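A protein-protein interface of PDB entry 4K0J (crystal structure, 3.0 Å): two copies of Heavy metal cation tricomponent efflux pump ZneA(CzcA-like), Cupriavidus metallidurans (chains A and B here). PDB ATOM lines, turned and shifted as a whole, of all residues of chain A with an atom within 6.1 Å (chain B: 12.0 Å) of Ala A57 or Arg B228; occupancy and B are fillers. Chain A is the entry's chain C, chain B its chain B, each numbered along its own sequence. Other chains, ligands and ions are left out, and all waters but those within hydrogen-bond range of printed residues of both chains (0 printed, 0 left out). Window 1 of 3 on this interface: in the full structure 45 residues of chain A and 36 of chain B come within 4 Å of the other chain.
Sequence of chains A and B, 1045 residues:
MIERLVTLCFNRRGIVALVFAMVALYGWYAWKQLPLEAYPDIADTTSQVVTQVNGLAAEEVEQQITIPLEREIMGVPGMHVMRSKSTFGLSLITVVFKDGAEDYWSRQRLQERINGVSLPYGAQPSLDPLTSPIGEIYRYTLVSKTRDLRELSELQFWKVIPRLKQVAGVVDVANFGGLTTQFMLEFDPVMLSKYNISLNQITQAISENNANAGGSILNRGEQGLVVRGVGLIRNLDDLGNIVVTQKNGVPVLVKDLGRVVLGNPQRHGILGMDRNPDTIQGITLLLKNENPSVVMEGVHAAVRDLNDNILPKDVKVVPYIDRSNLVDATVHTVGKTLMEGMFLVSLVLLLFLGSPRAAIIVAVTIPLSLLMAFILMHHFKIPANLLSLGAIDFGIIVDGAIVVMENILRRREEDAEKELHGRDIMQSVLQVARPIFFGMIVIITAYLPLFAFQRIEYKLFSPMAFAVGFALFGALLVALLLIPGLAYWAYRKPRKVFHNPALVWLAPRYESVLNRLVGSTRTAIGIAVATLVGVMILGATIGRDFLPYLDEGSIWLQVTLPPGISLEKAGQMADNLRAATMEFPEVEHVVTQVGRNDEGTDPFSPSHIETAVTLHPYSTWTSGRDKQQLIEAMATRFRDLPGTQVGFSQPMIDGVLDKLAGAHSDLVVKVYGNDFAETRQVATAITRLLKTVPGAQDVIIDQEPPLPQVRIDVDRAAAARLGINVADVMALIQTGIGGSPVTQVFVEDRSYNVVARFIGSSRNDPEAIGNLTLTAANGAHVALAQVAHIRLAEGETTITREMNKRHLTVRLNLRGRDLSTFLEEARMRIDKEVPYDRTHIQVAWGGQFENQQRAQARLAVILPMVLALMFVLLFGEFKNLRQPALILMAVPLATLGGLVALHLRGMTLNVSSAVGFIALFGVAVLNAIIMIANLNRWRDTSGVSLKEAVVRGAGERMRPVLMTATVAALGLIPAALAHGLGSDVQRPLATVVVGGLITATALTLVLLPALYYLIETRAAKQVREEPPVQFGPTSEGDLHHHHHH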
ATOM      1  N   VAL A  53       0.890  11.614   7.188  1.00  0.00           N
ATOM      2  CA  VAL A  53       0.888  10.153   7.188  1.00  0.00           C
ATOM      3  C   VAL A  53       1.568   9.618   8.455  1.00  0.00           C
ATOM      4  O   VAL A  53       2.793   9.649   8.577  1.00  0.00           O
ATOM      5  CB  VAL A  53       1.582   9.572   5.938  1.00  0.00           C
ATOM      6  CG1 VAL A  53       1.239   8.110   5.801  1.00  0.00           C
ATOM      7  CG2 VAL A  53       1.162  10.328   4.685  1.00  0.00           C
ATOM      8  N   GLY A  55       3.407   7.860  11.386  1.00  0.00           N
ATOM      9  CA  GLY A  55       4.404   6.825  11.606  1.00  0.00           C
ATOM     10  C   GLY A  55       5.322   6.536  10.430  1.00  0.00           C
ATOM     11  O   GLY A  55       6.249   5.730  10.540  1.00  0.00           O
ATOM     12  N   LEU A  56       5.069   7.201   9.306  1.00  0.00           N
ATOM     13  CA  LEU A  56       5.835   6.964   8.088  1.00  0.00           C
ATOM     14  C   LEU A  56       7.045   7.895   8.008  1.00  0.00           C
ATOM     15  O   LEU A  56       6.976   9.040   8.456  1.00  0.00           O
ATOM     16  CB  LEU A  56       4.933   7.127   6.860  1.00  0.00           C
ATOM     17  CG  LEU A  56       5.025   5.993   5.836  1.00  0.00           C
ATOM     18  CD1 LEU A  56       3.777   5.919   4.975  1.00  0.00           C
ATOM     19  CD2 LEU A  56       6.258   6.165   4.976  1.00  0.00           C
ATOM     20  N   ALA A  57       8.147   7.403   7.441  1.00  0.00           N
ATOM     21  CA  ALA A  57       9.388   8.176   7.361  1.00  0.00           C
ATOM     22  C   ALA A  57       9.446   9.204   6.212  1.00  0.00           C
ATOM     23  O   ALA A  57       8.441   9.470   5.543  1.00  0.00           O
ATOM     24  CB  ALA A  57      10.584   7.248   7.312  1.00  0.00           C
ATOM     25  N   ALA A  58      10.643   9.742   5.976  1.00  0.00           N
ATOM     26  CA  ALA A  58      10.823  11.020   5.273  1.00  0.00           C
ATOM     27  C   ALA A  58      11.181  10.986   3.780  1.00  0.00           C
ATOM     28  O   ALA A  58      11.801  11.922   3.272  1.00  0.00           O
ATOM     29  CB  ALA A  58      11.856  11.860   6.018  1.00  0.00           C
ATOM     30  N   GLU A  59      10.794   9.939   3.068  1.00  0.00           N
ATOM     31  CA  GLU A  59      11.153   9.854   1.657  1.00  0.00           C
ATOM     32  C   GLU A  59      10.038   9.187   0.868  1.00  0.00           C
ATOM     33  O   GLU A  59       9.933   9.320  -0.363  1.00  0.00           O
ATOM     34  CB  GLU A  59      12.473   9.098   1.486  1.00  0.00           C
ATOM     35  CG  GLU A  59      13.011   9.103   0.067  1.00  0.00           C
ATOM     36  CD  GLU A  59      13.100  10.500  -0.517  1.00  0.00           C
ATOM     37  OE1 GLU A  59      14.166  11.134  -0.357  1.00  0.00           O
ATOM     38  OE2 GLU A  59      12.108  10.960  -1.134  1.00  0.00           O
ATOM     39  N   GLU A  60       9.201   8.468   1.606  1.00  0.00           N
ATOM     40  CA  GLU A  60       7.973   7.909   1.073  1.00  0.00           C
ATOM     41  C   GLU A  60       6.865   8.914   1.369  1.00  0.00           C
ATOM     42  O   GLU A  60       5.695   8.553   1.493  1.00  0.00           O
ATOM     43  CB  GLU A  60       7.678   6.559   1.729  1.00  0.00           C
ATOM     44  CG  GLU A  60       8.782   6.057   2.671  1.00  0.00           C
ATOM     45  CD  GLU A  60       9.993   5.491   1.946  1.00  0.00           C
ATOM     46  OE1 GLU A  60      10.924   6.264   1.637  1.00  0.00           O
ATOM     47  OE2 GLU A  60      10.018   4.269   1.698  1.00  0.00           O
ATOM     48  N   VAL A  61       7.265  10.182   1.468  1.00  0.00           N
ATOM     49  CA  VAL A  61       6.394  11.281   1.864  1.00  0.00           C
ATOM     50  C   VAL A  61       6.637  12.503   0.968  1.00  0.00           C
ATOM     51  O   VAL A  61       5.889  13.483   1.013  1.00  0.00           O
ATOM     52  CB  VAL A  61       6.657  11.673   3.334  1.00  0.00           C
ATOM     53  CG1 VAL A  61       7.899  12.565   3.438  1.00  0.00           C
ATOM     54  CG2 VAL A  61       5.444  12.358   3.950  1.00  0.00           C
ATOM     55  N   THR A  87       8.947  15.204   5.385  1.00  0.00           N
ATOM     56  CA  THR A  87       9.626  14.542   6.492  1.00  0.00           C
ATOM     57  C   THR A  87       8.812  13.425   7.144  1.00  0.00           C
ATOM     58  O   THR A  87       7.651  13.188   6.796  1.00  0.00           O
ATOM     59  CB  THR A  87      10.011  15.556   7.598  1.00  0.00           C
ATOM     60  OG1 THR A  87      10.565  14.857   8.721  1.00  0.00           O
ATOM     61  CG2 THR A  87       8.787  16.337   8.047  1.00  0.00           C
ATOM     62  N   PHE A  88       9.453  12.747   8.094  1.00  0.00           N
ATOM     63  CA  PHE A  88       8.815  11.738   8.931  1.00  0.00           C
ATOM     64  C   PHE A  88       7.547  12.331   9.521  1.00  0.00           C
ATOM     65  O   PHE A  88       7.574  13.386  10.161  1.00  0.00           O
ATOM     66  CB  PHE A  88       9.782  11.292  10.040  1.00  0.00           C
ATOM     67  CG  PHE A  88       9.193  10.312  11.031  1.00  0.00           C
ATOM     68  CD1 PHE A  88       9.162   8.954  10.752  1.00  0.00           C
ATOM     69  CD2 PHE A  88       8.713  10.748  12.260  1.00  0.00           C
ATOM     70  CE1 PHE A  88       8.636   8.049  11.670  1.00  0.00           C
ATOM     71  CE2 PHE A  88       8.186   9.848  13.181  1.00  0.00           C
ATOM     72  CZ  PHE A  88       8.148   8.498  12.883  1.00  0.00           C
ATOM     73  N   GLY A  89       6.432  11.661   9.266  1.00  0.00           N
ATOM     74  CA  GLY A  89       5.151  12.138   9.733  1.00  0.00           C
ATOM     75  C   GLY A  89       4.320  12.807   8.656  1.00  0.00           C
ATOM     76  O   GLY A  89       3.118  12.550   8.567  1.00  0.00           O
ATOM     77  N   LEU A  90       4.939  13.648   7.825  1.00  0.00           N
ATOM     78  CA  LEU A  90       4.137  14.508   6.960  1.00  0.00           C
ATOM     79  C   LEU A  90       4.822  15.242   5.807  1.00  0.00           C
ATOM     80  O   LEU A  90       6.044  15.298   5.689  1.00  0.00           O
ATOM     81  CB  LEU A  90       3.416  15.560   7.808  1.00  0.00           C
ATOM     82  CG  LEU A  90       4.246  16.794   8.155  1.00  0.00           C
ATOM     83  CD1 LEU A  90       3.356  17.877   8.703  1.00  0.00           C
ATOM     84  CD2 LEU A  90       5.332  16.465   9.153  1.00  0.00           C
ATOM     85  N   GLN A 709      18.741   5.412  10.086  1.00  0.00           N
ATOM     86  CA  GLN A 709      17.440   4.788  10.189  1.00  0.00           C
ATOM     87  C   GLN A 709      17.696   3.304  10.072  1.00  0.00           C
ATOM     88  O   GLN A 709      18.412   2.872   9.176  1.00  0.00           O
ATOM     89  CB  GLN A 709      16.548   5.228   9.034  1.00  0.00           C
ATOM     90  CG  GLN A 709      16.455   6.731   8.849  1.00  0.00           C
ATOM     91  CD  GLN A 709      15.960   7.112   7.471  1.00  0.00           C
ATOM     92  OE1 GLN A 709      16.000   6.304   6.543  1.00  0.00           O
ATOM     93  NE2 GLN A 709      15.494   8.346   7.328  1.00  0.00           N
ATOM     94  N   VAL A 710      17.144   2.517  10.984  1.00  0.00           N
ATOM     95  CA  VAL A 710      17.177   1.081  10.796  1.00  0.00           C
ATOM     96  C   VAL A 710      16.160   0.765   9.699  1.00  0.00           C
ATOM     97  O   VAL A 710      14.952   0.901   9.889  1.00  0.00           O
ATOM     98  CB  VAL A 710      16.928   0.315  12.111  1.00  0.00           C
ATOM     99  CG1 VAL A 710      15.935   1.061  12.984  1.00  0.00           C
ATOM    100  CG2 VAL A 710      16.459  -1.102  11.825  1.00  0.00           C
ATOM    101  N   ARG A 711      16.676   0.399   8.533  1.00  0.00           N
ATOM    102  CA  ARG A 711      15.885   0.263   7.320  1.00  0.00           C
ATOM    103  C   ARG A 711      15.690  -1.193   6.933  1.00  0.00           C
ATOM    104  O   ARG A 711      16.650  -1.964   6.840  1.00  0.00           O
ATOM    105  CB  ARG A 711      16.586   1.004   6.186  1.00  0.00           C
ATOM    106  CG  ARG A 711      16.062   0.703   4.803  1.00  0.00           C
ATOM    107  CD  ARG A 711      16.749   1.587   3.785  1.00  0.00           C
ATOM    108  NE  ARG A 711      16.151   1.472   2.460  1.00  0.00           N
ATOM    109  CZ  ARG A 711      16.400   2.309   1.458  1.00  0.00           C
ATOM    110  NH1 ARG A 711      17.233   3.328   1.639  1.00  0.00           N
ATOM    111  NH2 ARG A 711      15.813   2.131   0.280  1.00  0.00           N
ATOM    112  N   ILE A 712      14.436  -1.567   6.700  1.00  0.00           N
ATOM    113  CA  ILE A 712      14.110  -2.936   6.307  1.00  0.00           C
ATOM    114  C   ILE A 712      13.637  -3.011   4.865  1.00  0.00           C
ATOM    115  O   ILE A 712      12.491  -2.716   4.570  1.00  0.00           O
ATOM    116  CB  ILE A 712      13.033  -3.545   7.220  1.00  0.00           C
ATOM    117  CG1 ILE A 712      13.458  -3.414   8.685  1.00  0.00           C
ATOM    118  CG2 ILE A 712      12.792  -4.997   6.838  1.00  0.00           C
ATOM    119  CD1 ILE A 712      12.320  -3.385   9.656  1.00  0.00           C
ATOM    120  N   ASP A 713      14.534  -3.394   3.965  1.00  0.00           N
ATOM    121  CA  ASP A 713      14.142  -3.629   2.586  1.00  0.00           C
ATOM    122  C   ASP A 713      13.691  -5.076   2.499  1.00  0.00           C
ATOM    123  O   ASP A 713      14.056  -5.884   3.342  1.00  0.00           O
ATOM    124  CB  ASP A 713      15.304  -3.354   1.633  1.00  0.00           C
ATOM    125  CG  ASP A 713      15.767  -1.905   1.677  1.00  0.00           C
ATOM    126  OD1 ASP A 713      16.827  -1.623   2.275  1.00  0.00           O
ATOM    127  OD2 ASP A 713      15.063  -1.043   1.116  1.00  0.00           O
ATOM    128  N   ILE A 733       5.588  -4.512  10.290  1.00  0.00           N
ATOM    129  CA  ILE A 733       6.308  -3.312  10.709  1.00  0.00           C
ATOM    130  C   ILE A 733       5.364  -2.208  11.146  1.00  0.00           C
ATOM    131  O   ILE A 733       5.658  -1.463  12.082  1.00  0.00           O
ATOM    132  CB  ILE A 733       7.196  -2.754   9.583  1.00  0.00           C
ATOM    133  CG1 ILE A 733       7.982  -3.875   8.908  1.00  0.00           C
ATOM    134  CG2 ILE A 733       8.152  -1.714  10.135  1.00  0.00           C
ATOM    135  CD1 ILE A 733       8.290  -3.617   7.447  1.00  0.00           C
ATOM    136  N   GLY A 795      19.492   8.363   6.080  1.00  0.00           N
ATOM    137  CA  GLY A 795      18.503   8.971   5.206  1.00  0.00           C
ATOM    138  C   GLY A 795      18.299  10.434   5.548  1.00  0.00           C
ATOM    139  O   GLY A 795      18.733  10.884   6.596  1.00  0.00           O
ATOM    140  N   GLU A 796      17.642  11.187   4.676  1.00  0.00           N
ATOM    141  CA  GLU A 796      17.435  12.607   4.941  1.00  0.00           C
ATOM    142  C   GLU A 796      16.323  12.833   5.964  1.00  0.00           C
ATOM    143  O   GLU A 796      15.340  12.104   5.990  1.00  0.00           O
ATOM    144  CB  GLU A 796      17.153  13.372   3.647  1.00  0.00           C
ATOM    145  CG  GLU A 796      17.236  14.887   3.799  1.00  0.00           C
ATOM    146  CD  GLU A 796      18.643  15.372   4.129  1.00  0.00           C
ATOM    147  OE1 GLU A 796      18.800  16.113   5.127  1.00  0.00           O
ATOM    148  OE2 GLU A 796      19.586  15.013   3.387  1.00  0.00           O
ATOM    149  N   ALA B 211       3.352  -1.059  -0.709  1.00  0.00           N
ATOM    150  CA  ALA B 211       3.141  -0.050   0.321  1.00  0.00           C
ATOM    151  C   ALA B 211       4.247  -0.090   1.370  1.00  0.00           C
ATOM    152  O   ALA B 211       4.413  -1.086   2.069  1.00  0.00           O
ATOM    153  CB  ALA B 211       1.779  -0.242   0.974  1.00  0.00           C
ATOM    154  N   ASN B 212       5.001   0.996   1.479  1.00  0.00           N
ATOM    155  CA  ASN B 212       6.049   1.086   2.485  1.00  0.00           C
ATOM    156  C   ASN B 212       5.496   1.208   3.896  1.00  0.00           C
ATOM    157  O   ASN B 212       4.298   1.414   4.087  1.00  0.00           O
ATOM    158  CB  ASN B 212       6.999   2.243   2.183  1.00  0.00           C
ATOM    159  CG  ASN B 212       7.872   1.971   0.978  1.00  0.00           C
ATOM    160  OD1 ASN B 212       7.960   0.839   0.507  1.00  0.00           O
ATOM    161  ND2 ASN B 212       8.523   3.009   0.473  1.00  0.00           N
ATOM    162  N   ALA B 213       6.369   1.072   4.885  1.00  0.00           N
ATOM    163  CA  ALA B 213       5.939   1.117   6.273  1.00  0.00           C
ATOM    164  C   ALA B 213       6.910   1.932   7.101  1.00  0.00           C
ATOM    165  O   ALA B 213       8.018   2.209   6.664  1.00  0.00           O
ATOM    166  CB  ALA B 213       5.806  -0.286   6.838  1.00  0.00           C
ATOM    167  N   GLY B 214       6.484   2.314   8.297  1.00  0.00           N
ATOM    168  CA  GLY B 214       7.301   3.118   9.181  1.00  0.00           C
ATOM    169  C   GLY B 214       7.046   2.734  10.619  1.00  0.00           C
ATOM    170  O   GLY B 214       5.998   3.062  11.176  1.00  0.00           O
ATOM    171  N   GLY B 215       8.003   2.038  11.223  1.00  0.00           N
ATOM    172  CA  GLY B 215       7.830   1.503  12.561  1.00  0.00           C
ATOM    173  C   GLY B 215       8.087   2.481  13.692  1.00  0.00           C
ATOM    174  O   GLY B 215       8.453   2.070  14.793  1.00  0.00           O
ATOM    175  N   SER B 216       7.883   3.769  13.426  1.00  0.00           N
ATOM    176  CA  SER B 216       8.137   4.828  14.404  1.00  0.00           C
ATOM    177  C   SER B 216       9.588   4.837  14.885  1.00  0.00           C
ATOM    178  O   SER B 216      10.493   4.414  14.165  1.00  0.00           O
ATOM    179  CB  SER B 216       7.181   4.725  15.596  1.00  0.00           C
ATOM    180  OG  SER B 216       7.460   3.574  16.372  1.00  0.00           O
ATOM    181  N   ILE B 217       9.807   5.309  16.105  1.00  0.00           N
ATOM    182  CA  ILE B 217      11.164   5.500  16.598  1.00  0.00           C
ATOM    183  C   ILE B 217      11.663   4.397  17.537  1.00  0.00           C
ATOM    184  O   ILE B 217      11.052   4.119  18.567  1.00  0.00           O
ATOM    185  CB  ILE B 217      11.313   6.854  17.308  1.00  0.00           C
ATOM    186  CG1 ILE B 217      10.948   8.008  16.364  1.00  0.00           C
ATOM    187  CG2 ILE B 217      12.718   7.003  17.839  1.00  0.00           C
ATOM    188  CD1 ILE B 217      10.789   9.362  17.068  1.00  0.00           C
ATOM    189  N   LEU B 218      12.779   3.773  17.163  1.00  0.00           N
ATOM    190  CA  LEU B 218      13.493   2.858  18.050  1.00  0.00           C
ATOM    191  C   LEU B 218      14.578   3.616  18.783  1.00  0.00           C
ATOM    192  O   LEU B 218      15.430   4.254  18.159  1.00  0.00           O
ATOM    193  CB  LEU B 218      14.151   1.720  17.275  1.00  0.00           C
ATOM    194  CG  LEU B 218      13.227   0.650  16.705  1.00  0.00           C
ATOM    195  CD1 LEU B 218      14.057  -0.558  16.305  1.00  0.00           C
ATOM    196  CD2 LEU B 218      12.139   0.274  17.711  1.00  0.00           C
ATOM    197  N   ASN B 219      14.546   3.540  20.108  1.00  0.00           N
ATOM    198  CA  ASN B 219      15.532   4.222  20.928  1.00  0.00           C
ATOM    199  C   ASN B 219      16.679   3.299  21.293  1.00  0.00           C
ATOM    200  O   ASN B 219      16.512   2.380  22.091  1.00  0.00           O
ATOM    201  CB  ASN B 219      14.885   4.778  22.193  1.00  0.00           C
ATOM    202  CG  ASN B 219      13.821   5.810  21.893  1.00  0.00           C
ATOM    203  OD1 ASN B 219      14.125   6.925  21.476  1.00  0.00           O
ATOM    204  ND2 ASN B 219      12.562   5.446  22.109  1.00  0.00           N
ATOM    205  N   GLY B 224      17.463   8.021  18.410  1.00  0.00           N
ATOM    206  CA  GLY B 224      16.151   7.502  18.078  1.00  0.00           C
ATOM    207  C   GLY B 224      15.965   7.383  16.580  1.00  0.00           C
ATOM    208  O   GLY B 224      15.628   8.350  15.902  1.00  0.00           O
ATOM    209  N   LEU B 225      16.178   6.178  16.070  1.00  0.00           N
ATOM    210  CA  LEU B 225      16.181   5.929  14.634  1.00  0.00           C
ATOM    211  C   LEU B 225      14.780   5.586  14.158  1.00  0.00           C
ATOM    212  O   LEU B 225      14.096   4.770  14.776  1.00  0.00           O
ATOM    213  CB  LEU B 225      17.090   4.747  14.323  1.00  0.00           C
ATOM    214  CG  LEU B 225      18.612   4.836  14.406  1.00  0.00           C
ATOM    215  CD1 LEU B 225      19.113   5.619  15.603  1.00  0.00           C
ATOM    216  CD2 LEU B 225      19.149   3.419  14.455  1.00  0.00           C
ATOM    217  N   VAL B 226      14.342   6.192  13.061  1.00  0.00           N
ATOM    218  CA  VAL B 226      13.026   5.846  12.540  1.00  0.00           C
ATOM    219  C   VAL B 226      13.145   4.543  11.770  1.00  0.00           C
ATOM    220  O   VAL B 226      14.209   4.232  11.237  1.00  0.00           O
ATOM    221  CB  VAL B 226      12.416   6.957  11.648  1.00  0.00           C
ATOM    222  CG1 VAL B 226      12.188   8.210  12.458  1.00  0.00           C
ATOM    223  CG2 VAL B 226      13.311   7.256  10.478  1.00  0.00           C
ATOM    224  N   VAL B 227      12.065   3.773  11.724  1.00  0.00           N
ATOM    225  CA  VAL B 227      12.092   2.498  11.013  1.00  0.00           C
ATOM    226  C   VAL B 227      11.554   2.650   9.595  1.00  0.00           C
ATOM    227  O   VAL B 227      10.462   3.167   9.386  1.00  0.00           O
ATOM    228  CB  VAL B 227      11.317   1.393  11.772  1.00  0.00           C
ATOM    229  CG1 VAL B 227      11.263   0.121  10.954  1.00  0.00           C
ATOM    230  CG2 VAL B 227      11.961   1.124  13.132  1.00  0.00           C
ATOM    231  N   ARG B 228      12.347   2.211   8.625  1.00  0.00           N
ATOM    232  CA  ARG B 228      11.981   2.299   7.217  1.00  0.00           C
ATOM    233  C   ARG B 228      11.659   0.928   6.623  1.00  0.00           C
ATOM    234  O   ARG B 228      12.560   0.150   6.309  1.00  0.00           O
ATOM    235  CB  ARG B 228      13.116   2.933   6.412  1.00  0.00           C
ATOM    236  CG  ARG B 228      13.134   4.448   6.412  1.00  0.00           C
ATOM    237  CD  ARG B 228      12.385   4.997   5.215  1.00  0.00           C
ATOM    238  NE  ARG B 228      13.050   4.716   3.947  1.00  0.00           N
ATOM    239  CZ  ARG B 228      13.932   5.528   3.375  1.00  0.00           C
ATOM    240  NH1 ARG B 228      14.480   5.203   2.212  1.00  0.00           N
ATOM    241  NH2 ARG B 228      14.265   6.668   3.964  1.00  0.00           N
ATOM    242  N   GLY B 229      10.370   0.638   6.478  1.00  0.00           N
ATOM    243  CA  GLY B 229       9.933  -0.524   5.726  1.00  0.00           C
ATOM    244  C   GLY B 229       9.833  -0.170   4.252  1.00  0.00           C
ATOM    245  O   GLY B 229       9.359   0.901   3.902  1.00  0.00           O
ATOM    246  N   VAL B 230      10.290  -1.057   3.380  1.00  0.00           N
ATOM    247  CA  VAL B 230      10.274  -0.774   1.955  1.00  0.00           C
ATOM    248  C   VAL B 230       9.583  -1.903   1.194  1.00  0.00           C
ATOM    249  O   VAL B 230      10.124  -3.002   1.075  1.00  0.00           O
ATOM    250  CB  VAL B 230      11.709  -0.556   1.405  1.00  0.00           C
ATOM    251  CG1 VAL B 230      11.698  -0.445  -0.116  1.00  0.00           C
ATOM    252  CG2 VAL B 230      12.335   0.678   2.020  1.00  0.00           C
ATOM    253  N   GLY B 231       8.388  -1.628   0.679  1.00  0.00           N
ATOM    254  CA  GLY B 231       7.620  -2.633  -0.030  1.00  0.00           C
ATOM    255  C   GLY B 231       7.268  -2.269  -1.460  1.00  0.00           C
ATOM    256  O   GLY B 231       6.785  -3.110  -2.219  1.00  0.00           O
ATOM    257  N   LEU B 232       7.504  -1.014  -1.825  1.00  0.00           N
ATOM    258  CA  LEU B 232       7.197  -0.513  -3.163  1.00  0.00           C
ATOM    259  C   LEU B 232       7.874  -1.328  -4.256  1.00  0.00           C
ATOM    260  O   LEU B 232       9.053  -1.655  -4.154  1.00  0.00           O
ATOM    261  CB  LEU B 232       7.639   0.944  -3.292  1.00  0.00           C
ATOM    262  CG  LEU B 232       6.647   2.075  -3.036  1.00  0.00           C
ATOM    263  CD1 LEU B 232       5.871   1.845  -1.757  1.00  0.00           C
ATOM    264  CD2 LEU B 232       7.403   3.389  -2.974  1.00  0.00           C
ATOM    265  N   ARG B 234       9.667  -1.451  -7.608  1.00  0.00           N
ATOM    266  CA  ARG B 234      10.464  -0.457  -8.304  1.00  0.00           C
ATOM    267  C   ARG B 234      10.504  -0.676  -9.812  1.00  0.00           C
ATOM    268  O   ARG B 234      10.769   0.256 -10.572  1.00  0.00           O
ATOM    269  CB  ARG B 234      11.881  -0.425  -7.731  1.00  0.00           C
ATOM    270  CG  ARG B 234      12.018   0.428  -6.489  1.00  0.00           C
ATOM    271  CD  ARG B 234      11.920   1.904  -6.837  1.00  0.00           C
ATOM    272  NE  ARG B 234      11.985   2.742  -5.644  1.00  0.00           N
ATOM    273  CZ  ARG B 234      10.926   3.112  -4.934  1.00  0.00           C
ATOM    274  NH1 ARG B 234       9.710   2.722  -5.302  1.00  0.00           N
ATOM    275  NH2 ARG B 234      11.079   3.871  -3.857  1.00  0.00           N
ATOM    276  N   GLU B 748      11.210   7.990  -9.237  1.00  0.00           N
ATOM    277  CA  GLU B 748      11.524   9.400  -9.031  1.00  0.00           C
ATOM    278  C   GLU B 748      10.245  10.195  -8.786  1.00  0.00           C
ATOM    279  O   GLU B 748       9.449   9.845  -7.920  1.00  0.00           O
ATOM    280  CB  GLU B 748      12.300   9.973 -10.219  1.00  0.00           C
ATOM    281  CG  GLU B 748      13.522   9.156 -10.632  1.00  0.00           C
ATOM    282  CD  GLU B 748      14.616   9.151  -9.581  1.00  0.00           C
ATOM    283  OE1 GLU B 748      14.595  10.022  -8.686  1.00  0.00           O
ATOM    284  OE2 GLU B 748      15.501   8.271  -9.650  1.00  0.00           O
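N of Gly B231 is in hydrogen-bond range of OD1 of Asn B212, 2.5 Å away.
The backbone NH (N) of Leu B232 is in hydrogen-bond range of the side-chain amide oxygen (OD1) of Asn B212 (3.0 Å).
The backbone NH of Gly B215 is in hydrogen-bond range of the backbone carbonyl oxygen of Val B227 (3.3 Å).
No position is printed for both chains.
O of Val B226 is in hydrogen-bond range of N of Val A710 (3.4 Å).
The side-chain carboxylate (OE1) of Glu A60 lies within salt-bridge range of the guanidinium group (NE) of Arg B228.
The side-chain amide oxygen (OE1) of Gln A709 sits at hydrogen-bond distance from the guanidinium group (NH2) of Arg B228, 3.1 Å away.
The backbone NH of Arg B228 is in hydrogen-bond range of the backbone carbonyl oxygen of Val A710, at 3.2 Å.
The backbone carbonyl oxygen (O) of Arg B228 sits at hydrogen-bond distance from the backbone NH (N) of Ile A712 (2.6 Å).
The backbone NH (N) of Val B230 lies within hydrogen-bond range of the backbone carbonyl oxygen (O) of Ile A712, 3.0 Å away.
O of Gly B214 sits close to O of Gly A55.
The side-chain carboxylate of Glu A60 lies close to the side-chain amide nitrogen of Asn B212.
The guanidinium group (NH1) of Arg B228 sits close to the guanidinium group (NH1) of Arg A711.
Among the printed residues, merely in contact across the chains: Asp A713 with Val B230 (3.3 Å), Gln A709 with Val B226 (3.4 Å), Val A710 with Val B227 (3.5 Å), Phe A88 with Val B226 (3.6 Å), Ile A712 with Gly B229 (3.6 Å), Ala A57 with Arg B228 (3.6 Å), Ile A733 with Val B227 (3.7 Å), Ile A733 with Gly B215 (3.7 Å), Gly A55 with Ser B216 (3.9 Å), Ile A712 with Val B227 (3.9 Å), Ile A733 with Gly B229 (3.9 Å), Glu A59 with Arg B228 (3.9 Å), Arg A711 with Val B230 (3.9 Å), Ile A733 with Ala B213 (3.9 Å) and Phe A88 with Ser B216 (3.97 Å).
Printed residues of chain A that touch a printed residue of chain B: Gly A55, Ala A57, Glu A59, Glu A60, Phe A88, Gln A709, Val A710, Arg A711, Ile A712, Asp A713 and Ile A733.
Hydrophobic or aromatic side chains of chain A that line the printed part of chain B: Ala A57, Phe A88, Val A710, Ile A712 and Ile A733.
Along chain B the printed residues that touch a printed residue of chain A span positions 212 to 230.
Among the printed residues, 24 pairs touch across the chains.
No residue of chain B comes within 4 Å of Val A61.
Printed residues of chain A within 4 Å of Gly B215: Ile A733.
Of the printed residues of chain A, Ser B216 touches Gly A55 (3.9 Å) and Phe A88 (3.97 Å).
Of chain A, only Ala A57 (3.6 Å), Glu A59 (3.9 Å), Glu A60 (3.5 Å), Gln A709 (3.1 Å), Val A710 (3.2 Å), Arg A711 (3.4 Å) and Ile A712 (2.6 Å) come within 4 Å of Arg B228.
Of the printed residues of chain A, Gly B229 touches Ile A712 and Ile A733.
The nearest residue of chain A that does not touch Arg B228 is Asp A713 (4.7 Å).
The nearest printed residue of chain B that does not touch Val A710 is Leu B225 (4.02 Å).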
